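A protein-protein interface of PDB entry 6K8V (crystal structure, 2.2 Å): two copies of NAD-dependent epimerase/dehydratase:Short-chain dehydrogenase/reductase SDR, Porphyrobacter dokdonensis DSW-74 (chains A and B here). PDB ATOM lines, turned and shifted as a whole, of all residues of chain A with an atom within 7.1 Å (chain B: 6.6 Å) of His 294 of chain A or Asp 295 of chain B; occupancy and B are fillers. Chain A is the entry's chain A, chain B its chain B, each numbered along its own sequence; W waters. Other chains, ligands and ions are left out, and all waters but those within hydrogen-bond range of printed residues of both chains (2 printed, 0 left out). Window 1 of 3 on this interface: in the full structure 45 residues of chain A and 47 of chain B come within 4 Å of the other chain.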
ATOM      1  N   SER A 202       0.345  -7.485 -24.418  1.00  0.00           N
ATOM      2  CA  SER A 202      -0.077  -6.069 -24.298  1.00  0.00           C
ATOM      3  C   SER A 202      -0.350  -5.511 -25.707  1.00  0.00           C
ATOM      4  O   SER A 202      -1.402  -4.878 -25.914  1.00  0.00           O
ATOM      5  CB  SER A 202       0.902  -5.270 -23.521  1.00  0.00           C
ATOM      6  OG  SER A 202       0.582  -3.888 -23.559  1.00  0.00           O
ATOM      7  N   SER A 206      -3.877  -4.237 -27.192  1.00  0.00           N
ATOM      8  CA  SER A 206      -3.830  -2.975 -27.961  1.00  0.00           C
ATOM      9  C   SER A 206      -4.781  -3.047 -29.152  1.00  0.00           C
ATOM     10  O   SER A 206      -5.401  -2.001 -29.481  1.00  0.00           O
ATOM     11  CB  SER A 206      -2.436  -2.715 -28.461  1.00  0.00           C
ATOM     12  OG  SER A 206      -2.228  -1.335 -28.520  1.00  0.00           O
ATOM     13  N   VAL A 216      -4.103   0.901 -24.712  1.00  0.00           N
ATOM     14  CA  VAL A 216      -3.250  -0.105 -24.024  1.00  0.00           C
ATOM     15  C   VAL A 216      -1.793   0.255 -24.334  1.00  0.00           C
ATOM     16  O   VAL A 216      -1.407   0.185 -25.491  1.00  0.00           O
ATOM     17  CB  VAL A 216      -3.631  -1.517 -24.491  1.00  0.00           C
ATOM     18  CG1 VAL A 216      -2.766  -2.592 -23.871  1.00  0.00           C
ATOM     19  CG2 VAL A 216      -5.102  -1.800 -24.267  1.00  0.00           C
ATOM     20  N   ASN A 217      -1.009   0.554 -23.305  1.00  0.00           N
ATOM     21  CA  ASN A 217       0.402   1.004 -23.446  1.00  0.00           C
ATOM     22  C   ASN A 217       1.305   0.289 -22.435  1.00  0.00           C
ATOM     23  O   ASN A 217       0.836  -0.128 -21.347  1.00  0.00           O
ATOM     24  CB  ASN A 217       0.473   2.525 -23.333  1.00  0.00           C
ATOM     25  CG  ASN A 217      -0.250   3.187 -24.485  1.00  0.00           C
ATOM     26  OD1 ASN A 217       0.213   3.132 -25.622  1.00  0.00           O
ATOM     27  ND2 ASN A 217      -1.402   3.779 -24.201  1.00  0.00           N
ATOM     28  N   LEU A 218       2.593   0.228 -22.770  1.00  0.00           N
ATOM     29  CA  LEU A 218       3.571  -0.688 -22.144  1.00  0.00           C
ATOM     30  C   LEU A 218       4.719   0.152 -21.571  1.00  0.00           C
ATOM     31  O   LEU A 218       5.396   0.868 -22.357  1.00  0.00           O
ATOM     32  CB  LEU A 218       4.005  -1.643 -23.251  1.00  0.00           C
ATOM     33  CG  LEU A 218       4.661  -2.950 -22.844  1.00  0.00           C
ATOM     34  CD1 LEU A 218       3.834  -3.686 -21.803  1.00  0.00           C
ATOM     35  CD2 LEU A 218       4.863  -3.829 -24.085  1.00  0.00           C
ATOM     36  N   VAL A 219       4.881   0.123 -20.246  1.00  0.00           N
ATOM     37  CA  VAL A 219       6.008   0.791 -19.545  1.00  0.00           C
ATOM     38  C   VAL A 219       7.130  -0.226 -19.325  1.00  0.00           C
ATOM     39  O   VAL A 219       6.884  -1.290 -18.695  1.00  0.00           O
ATOM     40  CB  VAL A 219       5.588   1.446 -18.223  1.00  0.00           C
ATOM     41  CG1 VAL A 219       6.772   2.159 -17.587  1.00  0.00           C
ATOM     42  CG2 VAL A 219       4.443   2.407 -18.418  1.00  0.00           C
ATOM     43  N   TYR A 220       8.318   0.130 -19.811  1.00  0.00           N
ATOM     44  CA  TYR A 220       9.586  -0.626 -19.666  1.00  0.00           C
ATOM     45  C   TYR A 220      10.513   0.180 -18.752  1.00  0.00           C
ATOM     46  O   TYR A 220      11.308   1.020 -19.201  1.00  0.00           O
ATOM     47  CB  TYR A 220      10.221  -0.888 -21.033  1.00  0.00           C
ATOM     48  CG  TYR A 220       9.577  -1.893 -21.963  1.00  0.00           C
ATOM     49  CD1 TYR A 220       9.894  -3.238 -21.894  1.00  0.00           C
ATOM     50  CD2 TYR A 220       8.795  -1.475 -23.033  1.00  0.00           C
ATOM     51  CE1 TYR A 220       9.399  -4.141 -22.818  1.00  0.00           C
ATOM     52  CE2 TYR A 220       8.273  -2.364 -23.955  1.00  0.00           C
ATOM     53  CZ  TYR A 220       8.583  -3.706 -23.850  1.00  0.00           C
ATOM     54  OH  TYR A 220       8.079  -4.602 -24.752  1.00  0.00           O
ATOM     55  N   LEU A 283       0.344   8.772 -18.984  1.00  0.00           N
ATOM     56  CA  LEU A 283      -0.430   7.698 -19.658  1.00  0.00           C
ATOM     57  C   LEU A 283      -1.834   7.529 -19.068  1.00  0.00           C
ATOM     58  O   LEU A 283      -2.735   7.149 -19.848  1.00  0.00           O
ATOM     59  CB  LEU A 283       0.378   6.397 -19.577  1.00  0.00           C
ATOM     60  CG  LEU A 283       1.682   6.408 -20.379  1.00  0.00           C
ATOM     61  CD1 LEU A 283       2.390   5.063 -20.328  1.00  0.00           C
ATOM     62  CD2 LEU A 283       1.414   6.807 -21.825  1.00  0.00           C
ATOM     63  N   ALA A 290      -3.937  10.092 -27.522  1.00  0.00           N
ATOM     64  CA  ALA A 290      -3.516   9.760 -28.901  1.00  0.00           C
ATOM     65  C   ALA A 290      -2.654   8.482 -28.988  1.00  0.00           C
ATOM     66  O   ALA A 290      -2.481   7.999 -30.111  1.00  0.00           O
ATOM     67  CB  ALA A 290      -2.802  10.946 -29.502  1.00  0.00           C
ATOM     68  N   TYR A 291      -2.119   7.939 -27.896  1.00  0.00           N
ATOM     69  CA  TYR A 291      -1.164   6.809 -27.945  1.00  0.00           C
ATOM     70  C   TYR A 291      -1.898   5.478 -27.756  1.00  0.00           C
ATOM     71  O   TYR A 291      -2.643   5.404 -26.770  1.00  0.00           O
ATOM     72  CB  TYR A 291      -0.143   6.926 -26.818  1.00  0.00           C
ATOM     73  CG  TYR A 291       0.813   8.090 -26.891  1.00  0.00           C
ATOM     74  CD1 TYR A 291       0.519   9.308 -26.313  1.00  0.00           C
ATOM     75  CD2 TYR A 291       2.051   7.957 -27.486  1.00  0.00           C
ATOM     76  CE1 TYR A 291       1.417  10.367 -26.352  1.00  0.00           C
ATOM     77  CE2 TYR A 291       2.955   9.011 -27.536  1.00  0.00           C
ATOM     78  CZ  TYR A 291       2.655  10.219 -26.951  1.00  0.00           C
ATOM     79  OH  TYR A 291       3.559  11.252 -26.996  1.00  0.00           O
ATOM     80  N   ASN A 292      -1.615   4.452 -28.570  1.00  0.00           N
ATOM     81  CA  ASN A 292      -2.081   3.048 -28.353  1.00  0.00           C
ATOM     82  C   ASN A 292      -0.961   2.113 -28.835  1.00  0.00           C
ATOM     83  O   ASN A 292      -0.305   2.454 -29.830  1.00  0.00           O
ATOM     84  CB  ASN A 292      -3.449   2.765 -29.000  1.00  0.00           C
ATOM     85  CG  ASN A 292      -3.993   1.368 -28.712  1.00  0.00           C
ATOM     86  OD1 ASN A 292      -4.050   0.925 -27.565  1.00  0.00           O
ATOM     87  ND2 ASN A 292      -4.413   0.648 -29.740  1.00  0.00           N
ATOM     88  N   GLY A 293      -0.754   0.989 -28.136  1.00  0.00           N
ATOM     89  CA  GLY A 293       0.248  -0.062 -28.423  1.00  0.00           C
ATOM     90  C   GLY A 293       1.668   0.479 -28.373  1.00  0.00           C
ATOM     91  O   GLY A 293       2.543  -0.074 -29.076  1.00  0.00           O
ATOM     92  N   HIS A 294       1.881   1.545 -27.608  1.00  0.00           N
ATOM     93  CA  HIS A 294       3.135   2.329 -27.584  1.00  0.00           C
ATOM     94  C   HIS A 294       4.028   1.893 -26.402  1.00  0.00           C
ATOM     95  O   HIS A 294       3.462   1.587 -25.320  1.00  0.00           O
ATOM     96  CB  HIS A 294       2.768   3.814 -27.579  1.00  0.00           C
ATOM     97  CG  HIS A 294       3.911   4.690 -27.926  1.00  0.00           C
ATOM     98  ND1 HIS A 294       3.949   5.452 -29.070  1.00  0.00           N
ATOM     99  CD2 HIS A 294       5.071   4.901 -27.297  1.00  0.00           C
ATOM    100  CE1 HIS A 294       5.068   6.138 -29.103  1.00  0.00           C
ATOM    101  NE2 HIS A 294       5.765   5.819 -28.043  1.00  0.00           N
ATOM    102  N   ASP A 295       5.358   1.861 -26.597  1.00  0.00           N
ATOM    103  CA  ASP A 295       6.348   1.541 -25.543  1.00  0.00           C
ATOM    104  C   ASP A 295       6.858   2.837 -24.896  1.00  0.00           C
ATOM    105  O   ASP A 295       7.132   3.812 -25.636  1.00  0.00           O
ATOM    106  CB  ASP A 295       7.512   0.717 -26.091  1.00  0.00           C
ATOM    107  CG  ASP A 295       7.071  -0.603 -26.713  1.00  0.00           C
ATOM    108  OD1 ASP A 295       5.954  -1.048 -26.467  1.00  0.00           O
ATOM    109  OD2 ASP A 295       7.855  -1.164 -27.459  1.00  0.00           O
ATOM    110  N   PHE A 296       6.987   2.834 -23.562  1.00  0.00           N
ATOM    111  CA  PHE A 296       7.641   3.901 -22.757  1.00  0.00           C
ATOM    112  C   PHE A 296       8.803   3.287 -21.963  1.00  0.00           C
ATOM    113  O   PHE A 296       8.604   2.662 -20.901  1.00  0.00           O
ATOM    114  CB  PHE A 296       6.582   4.597 -21.912  1.00  0.00           C
ATOM    115  CG  PHE A 296       5.565   5.275 -22.785  1.00  0.00           C
ATOM    116  CD1 PHE A 296       4.533   4.546 -23.355  1.00  0.00           C
ATOM    117  CD2 PHE A 296       5.681   6.628 -23.091  1.00  0.00           C
ATOM    118  CE1 PHE A 296       3.606   5.166 -24.176  1.00  0.00           C
ATOM    119  CE2 PHE A 296       4.767   7.249 -23.931  1.00  0.00           C
ATOM    120  CZ  PHE A 296       3.727   6.516 -24.474  1.00  0.00           C
ATOM    121  N   GLU A 297       9.998   3.424 -22.539  1.00  0.00           N
ATOM    122  CA  GLU A 297      11.246   2.852 -21.977  1.00  0.00           C
ATOM    123  C   GLU A 297      11.942   3.887 -21.095  1.00  0.00           C
ATOM    124  O   GLU A 297      12.657   4.706 -21.630  1.00  0.00           O
ATOM    125  CB  GLU A 297      12.151   2.360 -23.109  1.00  0.00           C
ATOM    126  CG  GLU A 297      11.416   1.556 -24.162  1.00  0.00           C
ATOM    127  CD  GLU A 297      12.245   0.933 -25.267  1.00  0.00           C
ATOM    128  OE1 GLU A 297      11.668   0.355 -26.169  1.00  0.00           O
ATOM    129  OE2 GLU A 297      13.446   1.028 -25.218  1.00  0.00           O
ATOM    130  N   ARG B 182       7.844   7.363 -42.492  1.00  0.00           N
ATOM    131  CA  ARG B 182       7.954   5.899 -42.339  1.00  0.00           C
ATOM    132  C   ARG B 182       6.895   5.194 -43.183  1.00  0.00           C
ATOM    133  O   ARG B 182       6.873   3.954 -43.156  1.00  0.00           O
ATOM    134  CB  ARG B 182       7.854   5.574 -40.850  1.00  0.00           C
ATOM    135  CG  ARG B 182       9.187   5.745 -40.138  1.00  0.00           C
ATOM    136  CD  ARG B 182       9.029   5.994 -38.662  1.00  0.00           C
ATOM    137  NE  ARG B 182       8.977   4.762 -37.901  1.00  0.00           N
ATOM    138  CZ  ARG B 182       9.175   4.678 -36.582  1.00  0.00           C
ATOM    139  NH1 ARG B 182       9.453   5.757 -35.865  1.00  0.00           N
ATOM    140  NH2 ARG B 182       9.116   3.503 -35.979  1.00  0.00           N
ATOM    141  N   ASN B 199      15.298  11.738 -38.479  1.00  0.00           N
ATOM    142  CA  ASN B 199      14.967  10.683 -37.500  1.00  0.00           C
ATOM    143  C   ASN B 199      16.284  10.116 -36.950  1.00  0.00           C
ATOM    144  O   ASN B 199      16.455  10.145 -35.714  1.00  0.00           O
ATOM    145  CB  ASN B 199      14.054   9.608 -38.090  1.00  0.00           C
ATOM    146  CG  ASN B 199      12.666  10.090 -38.448  1.00  0.00           C
ATOM    147  OD1 ASN B 199      12.183  11.101 -37.947  1.00  0.00           O
ATOM    148  ND2 ASN B 199      12.003   9.353 -39.322  1.00  0.00           N
ATOM    149  N   ASN B 217      14.843  13.735 -27.789  1.00  0.00           N
ATOM    150  CA  ASN B 217      13.652  12.883 -28.039  1.00  0.00           C
ATOM    151  C   ASN B 217      12.954  13.341 -29.317  1.00  0.00           C
ATOM    152  O   ASN B 217      13.043  14.540 -29.700  1.00  0.00           O
ATOM    153  CB  ASN B 217      12.790  12.778 -26.787  1.00  0.00           C
ATOM    154  CG  ASN B 217      13.529  12.047 -25.683  1.00  0.00           C
ATOM    155  OD1 ASN B 217      13.878  10.864 -25.819  1.00  0.00           O
ATOM    156  ND2 ASN B 217      13.773  12.753 -24.592  1.00  0.00           N
ATOM    157  N   LEU B 218      12.335  12.374 -29.976  1.00  0.00           N
ATOM    158  CA  LEU B 218      11.780  12.486 -31.355  1.00  0.00           C
ATOM    159  C   LEU B 218      10.259  12.294 -31.285  1.00  0.00           C
ATOM    160  O   LEU B 218       9.809  11.171 -30.885  1.00  0.00           O
ATOM    161  CB  LEU B 218      12.451  11.379 -32.180  1.00  0.00           C
ATOM    162  CG  LEU B 218      12.290  11.468 -33.688  1.00  0.00           C
ATOM    163  CD1 LEU B 218      12.912  12.753 -34.197  1.00  0.00           C
ATOM    164  CD2 LEU B 218      12.922  10.251 -34.359  1.00  0.00           C
ATOM    165  N   VAL B 219       9.491  13.317 -31.643  1.00  0.00           N
ATOM    166  CA  VAL B 219       8.003  13.238 -31.726  1.00  0.00           C
ATOM    167  C   VAL B 219       7.586  12.920 -33.178  1.00  0.00           C
ATOM    168  O   VAL B 219       7.881  13.720 -34.085  1.00  0.00           O
ATOM    169  CB  VAL B 219       7.353  14.549 -31.250  1.00  0.00           C
ATOM    170  CG1 VAL B 219       5.833  14.487 -31.338  1.00  0.00           C
ATOM    171  CG2 VAL B 219       7.772  14.919 -29.848  1.00  0.00           C
ATOM    172  N   TYR B 220       6.807  11.859 -33.350  1.00  0.00           N
ATOM    173  CA  TYR B 220       6.249  11.549 -34.683  1.00  0.00           C
ATOM    174  C   TYR B 220       4.751  11.841 -34.657  1.00  0.00           C
ATOM    175  O   TYR B 220       3.979  10.954 -34.346  1.00  0.00           O
ATOM    176  CB  TYR B 220       6.380  10.056 -34.960  1.00  0.00           C
ATOM    177  CG  TYR B 220       7.769   9.585 -35.274  1.00  0.00           C
ATOM    178  CD1 TYR B 220       8.645   9.226 -34.272  1.00  0.00           C
ATOM    179  CD2 TYR B 220       8.193   9.469 -36.582  1.00  0.00           C
ATOM    180  CE1 TYR B 220       9.914   8.766 -34.558  1.00  0.00           C
ATOM    181  CE2 TYR B 220       9.460   9.014 -36.888  1.00  0.00           C
ATOM    182  CZ  TYR B 220      10.328   8.675 -35.872  1.00  0.00           C
ATOM    183  OH  TYR B 220      11.564   8.220 -36.184  1.00  0.00           O
ATOM    184  N   GLY B 293      16.771   9.435 -26.552  1.00  0.00           N
ATOM    185  CA  GLY B 293      16.730   8.806 -27.884  1.00  0.00           C
ATOM    186  C   GLY B 293      15.471   7.996 -28.047  1.00  0.00           C
ATOM    187  O   GLY B 293      15.523   6.910 -28.662  1.00  0.00           O
ATOM    188  N   HIS B 294      14.403   8.485 -27.429  1.00  0.00           N
ATOM    189  CA  HIS B 294      13.092   7.805 -27.358  1.00  0.00           C
ATOM    190  C   HIS B 294      12.178   8.468 -28.375  1.00  0.00           C
ATOM    191  O   HIS B 294      12.302   9.707 -28.578  1.00  0.00           O
ATOM    192  CB  HIS B 294      12.522   7.836 -25.942  1.00  0.00           C
ATOM    193  CG  HIS B 294      11.345   6.944 -25.774  1.00  0.00           C
ATOM    194  ND1 HIS B 294      11.418   5.731 -25.121  1.00  0.00           N
ATOM    195  CD2 HIS B 294      10.063   7.092 -26.135  1.00  0.00           C
ATOM    196  CE1 HIS B 294      10.237   5.162 -25.118  1.00  0.00           C
ATOM    197  NE2 HIS B 294       9.397   5.957 -25.753  1.00  0.00           N
ATOM    198  N   ASP B 295      11.324   7.646 -28.975  1.00  0.00           N
ATOM    199  CA  ASP B 295      10.308   8.008 -30.004  1.00  0.00           C
ATOM    200  C   ASP B 295       8.945   8.191 -29.342  1.00  0.00           C
ATOM    201  O   ASP B 295       8.523   7.307 -28.600  1.00  0.00           O
ATOM    202  CB  ASP B 295      10.207   6.909 -31.071  1.00  0.00           C
ATOM    203  CG  ASP B 295      11.470   6.733 -31.896  1.00  0.00           C
ATOM    204  OD1 ASP B 295      12.297   7.707 -31.928  1.00  0.00           O
ATOM    205  OD2 ASP B 295      11.623   5.638 -32.489  1.00  0.00           O
ATOM    206  N   PHE B 296       8.241   9.258 -29.688  1.00  0.00           N
ATOM    207  CA  PHE B 296       6.860   9.515 -29.227  1.00  0.00           C
ATOM    208  C   PHE B 296       5.964   9.668 -30.453  1.00  0.00           C
ATOM    209  O   PHE B 296       5.942  10.747 -31.093  1.00  0.00           O
ATOM    210  CB  PHE B 296       6.872  10.714 -28.285  1.00  0.00           C
ATOM    211  CG  PHE B 296       7.684  10.456 -27.042  1.00  0.00           C
ATOM    212  CD1 PHE B 296       9.056  10.681 -27.028  1.00  0.00           C
ATOM    213  CD2 PHE B 296       7.071  10.006 -25.882  1.00  0.00           C
ATOM    214  CE1 PHE B 296       9.800  10.455 -25.884  1.00  0.00           C
ATOM    215  CE2 PHE B 296       7.818   9.782 -24.736  1.00  0.00           C
ATOM    216  CZ  PHE B 296       9.176  10.015 -24.738  1.00  0.00           C
ATOM    217  N   GLU B 297       5.276   8.580 -30.776  1.00  0.00           N
ATOM    218  CA  GLU B 297       4.437   8.398 -31.987  1.00  0.00           C
ATOM    219  C   GLU B 297       2.990   8.681 -31.593  1.00  0.00           C
ATOM    220  O   GLU B 297       2.346   7.785 -31.028  1.00  0.00           O
ATOM    221  CB  GLU B 297       4.616   6.990 -32.550  1.00  0.00           C
ATOM    222  CG  GLU B 297       6.061   6.654 -32.918  1.00  0.00           C
ATOM    223  CD  GLU B 297       6.286   5.222 -33.401  1.00  0.00           C
ATOM    224  OE1 GLU B 297       7.339   4.685 -33.125  1.00  0.00           O
ATOM    225  OE2 GLU B 297       5.408   4.654 -34.062  1.00  0.00           O
ATOM    226  N   VAL B 298       2.553   9.917 -31.833  1.00  0.00           N
ATOM    227  CA  VAL B 298       1.222  10.476 -31.482  1.00  0.00           C
ATOM    228  C   VAL B 298       0.328  10.239 -32.695  1.00  0.00           C
ATOM    229  O   VAL B 298       0.034  11.191 -33.438  1.00  0.00           O
ATOM    230  CB  VAL B 298       1.332  11.973 -31.125  1.00  0.00           C
ATOM    231  CG1 VAL B 298       0.150  12.417 -30.265  1.00  0.00           C
ATOM    232  CG2 VAL B 298       2.625  12.290 -30.405  1.00  0.00           C
ATOM    233  N   THR B 299      -0.035   8.984 -32.912  1.00  0.00           N
ATOM    234  CA  THR B 299      -0.572   8.491 -34.189  1.00  0.00           C
ATOM    235  C   THR B 299      -1.867   7.670 -34.045  1.00  0.00           C
ATOM    236  O   THR B 299      -2.288   7.139 -35.074  1.00  0.00           O
ATOM    237  CB  THR B 299       0.469   7.583 -34.852  1.00  0.00           C
ATOM    238  OG1 THR B 299       0.626   6.420 -34.043  1.00  0.00           O
ATOM    239  CG2 THR B 299       1.791   8.270 -35.089  1.00  0.00           C
ATOM    240  N   GLY B 301      -1.938   4.797 -32.644  1.00  0.00           N
ATOM    241  CA  GLY B 301      -1.422   3.418 -32.794  1.00  0.00           C
ATOM    242  C   GLY B 301      -1.197   3.002 -34.249  1.00  0.00           C
ATOM    243  O   GLY B 301      -1.496   1.852 -34.573  1.00  0.00           O
ATOM    244  N   LYS B 306      10.073   0.359 -37.371  1.00  0.00           N
ATOM    245  CA  LYS B 306      11.224   1.302 -37.254  1.00  0.00           C
ATOM    246  C   LYS B 306      12.182   1.088 -38.438  1.00  0.00           C
ATOM    247  O   LYS B 306      12.692   2.103 -38.974  1.00  0.00           O
ATOM    248  CB  LYS B 306      11.921   1.119 -35.902  1.00  0.00           C
ATOM    249  CG  LYS B 306      11.191   1.738 -34.715  1.00  0.00           C
ATOM    250  CD  LYS B 306      11.624   1.227 -33.353  1.00  0.00           C
ATOM    251  CE  LYS B 306      13.103   1.391 -33.063  1.00  0.00           C
ATOM    252  NZ  LYS B 306      13.486   2.811 -32.878  1.00  0.00           N
HETATM  253  O   HOH W   1       0.333   5.264 -30.642  1.00  0.00           O
HETATM  254  O   HOH W   2       8.180   4.420 -29.013  1.00  0.00           O
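Of the printed residues of chain B, His 294 of chain A touches Asp 295 (3.2 Å), Phe 296 (3.8 Å) and Glu 297 (3.0 Å). Printed residues of chain A within 4 Å of Val 298 of chain B: Ala 290 and Tyr 291. Of the printed residues of chain A, Phe 296 of chain B touches Tyr 291 (3.6 Å) and His 294 (3.8 Å). Of the printed residues of chain B, Asp 295 of chain A touches His 294. Of the printed residues of chain B, Tyr 291 of chain A touches Phe 296, Glu 297 and Val 298. Printed residues of chain A within 4 Å of Gly 301 of chain B: Asn 292. The nearest printed residue of chain B that does not touch Asp 295 of chain A is Asp 295 of chain B (4.8 Å).
Of the 15 printed residues of chain B, 7 touch a printed residue of chain A. Along chain B the printed residues that touch a printed residue of chain A span positions 294 to 301. Among the printed residues, 12 pairs touch across the chains. Among the printed residues, no Asp or Glu carboxylate lies within 4 Å of a Lys or Arg side-chain nitrogen of the other chain.
The side-chain amide nitrogen (ND2) of Asn 292 of chain A lies within hydrogen-bond range of the backbone carbonyl oxygen (O) of Ser 206 of chain A (2.8 Å). The side-chain amide oxygen of Asn 292 of chain A lies within hydrogen-bond range of the backbone NH of Val 216 of chain A (2.9 Å). The backbone NH (N) of Tyr 220 of chain A sits at hydrogen-bond distance from the backbone carbonyl oxygen (O) of Phe 296 of chain A (2.8 Å). OE1 of Glu 297 of chain B lies within salt-bridge range of NH2 of Arg 182 of chain B. OD1 of Asn 217 of chain B is in hydrogen-bond range of N of His 294 of chain B, at 2.9 Å. OG1 of Thr 299 of chain B lies close to N of Gly 301 of chain B (3.3 Å).
Val 298 of chain B touches Ala 290 of chain A (CG1 to CB, 3.4 Å). Ala 290 of chain A touches Thr 299 of chain B. Phe 296 of chain B touches Tyr 291 of chain A (CB to OH, 3.6 Å). Tyr 291 of chain A touches Glu 297 of chain B (CD2 to O, 3.6 Å). CG2 of Val 298 of chain B touches OH of Tyr 291 of chain A, 3.7 Å away. Asn 292 of chain A touches Gly 301 of chain B. CE1 of His 294 of chain A touches CA of Phe 296 of chain B, 3.8 Å away. CA of Phe 296 of chain A touches CE1 of His 294 of chain B, at 3.7 Å. N of Glu 297 of chain A touches CE1 of His 294 of chain B (3.1 Å).
A ring nitrogen (NE2) of His 294 of chain A is in hydrogen-bond range of the backbone carbonyl oxygen of Asp 295 of chain B. ND1 of His 294 of chain A is in hydrogen-bond range of O of Glu 297 of chain B, 3.4 Å away. NE2 of His 294 of chain B sits at hydrogen-bond distance from O of Asp 295 of chain A.
His 294 of chain A touches Asp 295 of chain B, and with the chains exchanged Asp 295 of chain A touches His 294 of chain B. His 294 of chain A touches Phe 296 of chain B, and with the chains exchanged Phe 296 of chain A touches His 294 of chain B. His 294 of chain A touches Glu 297 of chain B, and with the chains exchanged Glu 297 of chain A touches His 294 of chain B.
Water W2 bridges O of Asp 295 of chain B (2.9 Å) and NE2 of His 294 of chain A (3.0 Å). Water W1 lies within hydrogen-bond range of the backbone NH (N) of Asn 292 of chain A, the backbone NH (N) of Gly 301 of chain B and the backbone carbonyl oxygen (O) of Glu 297 of chain B.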
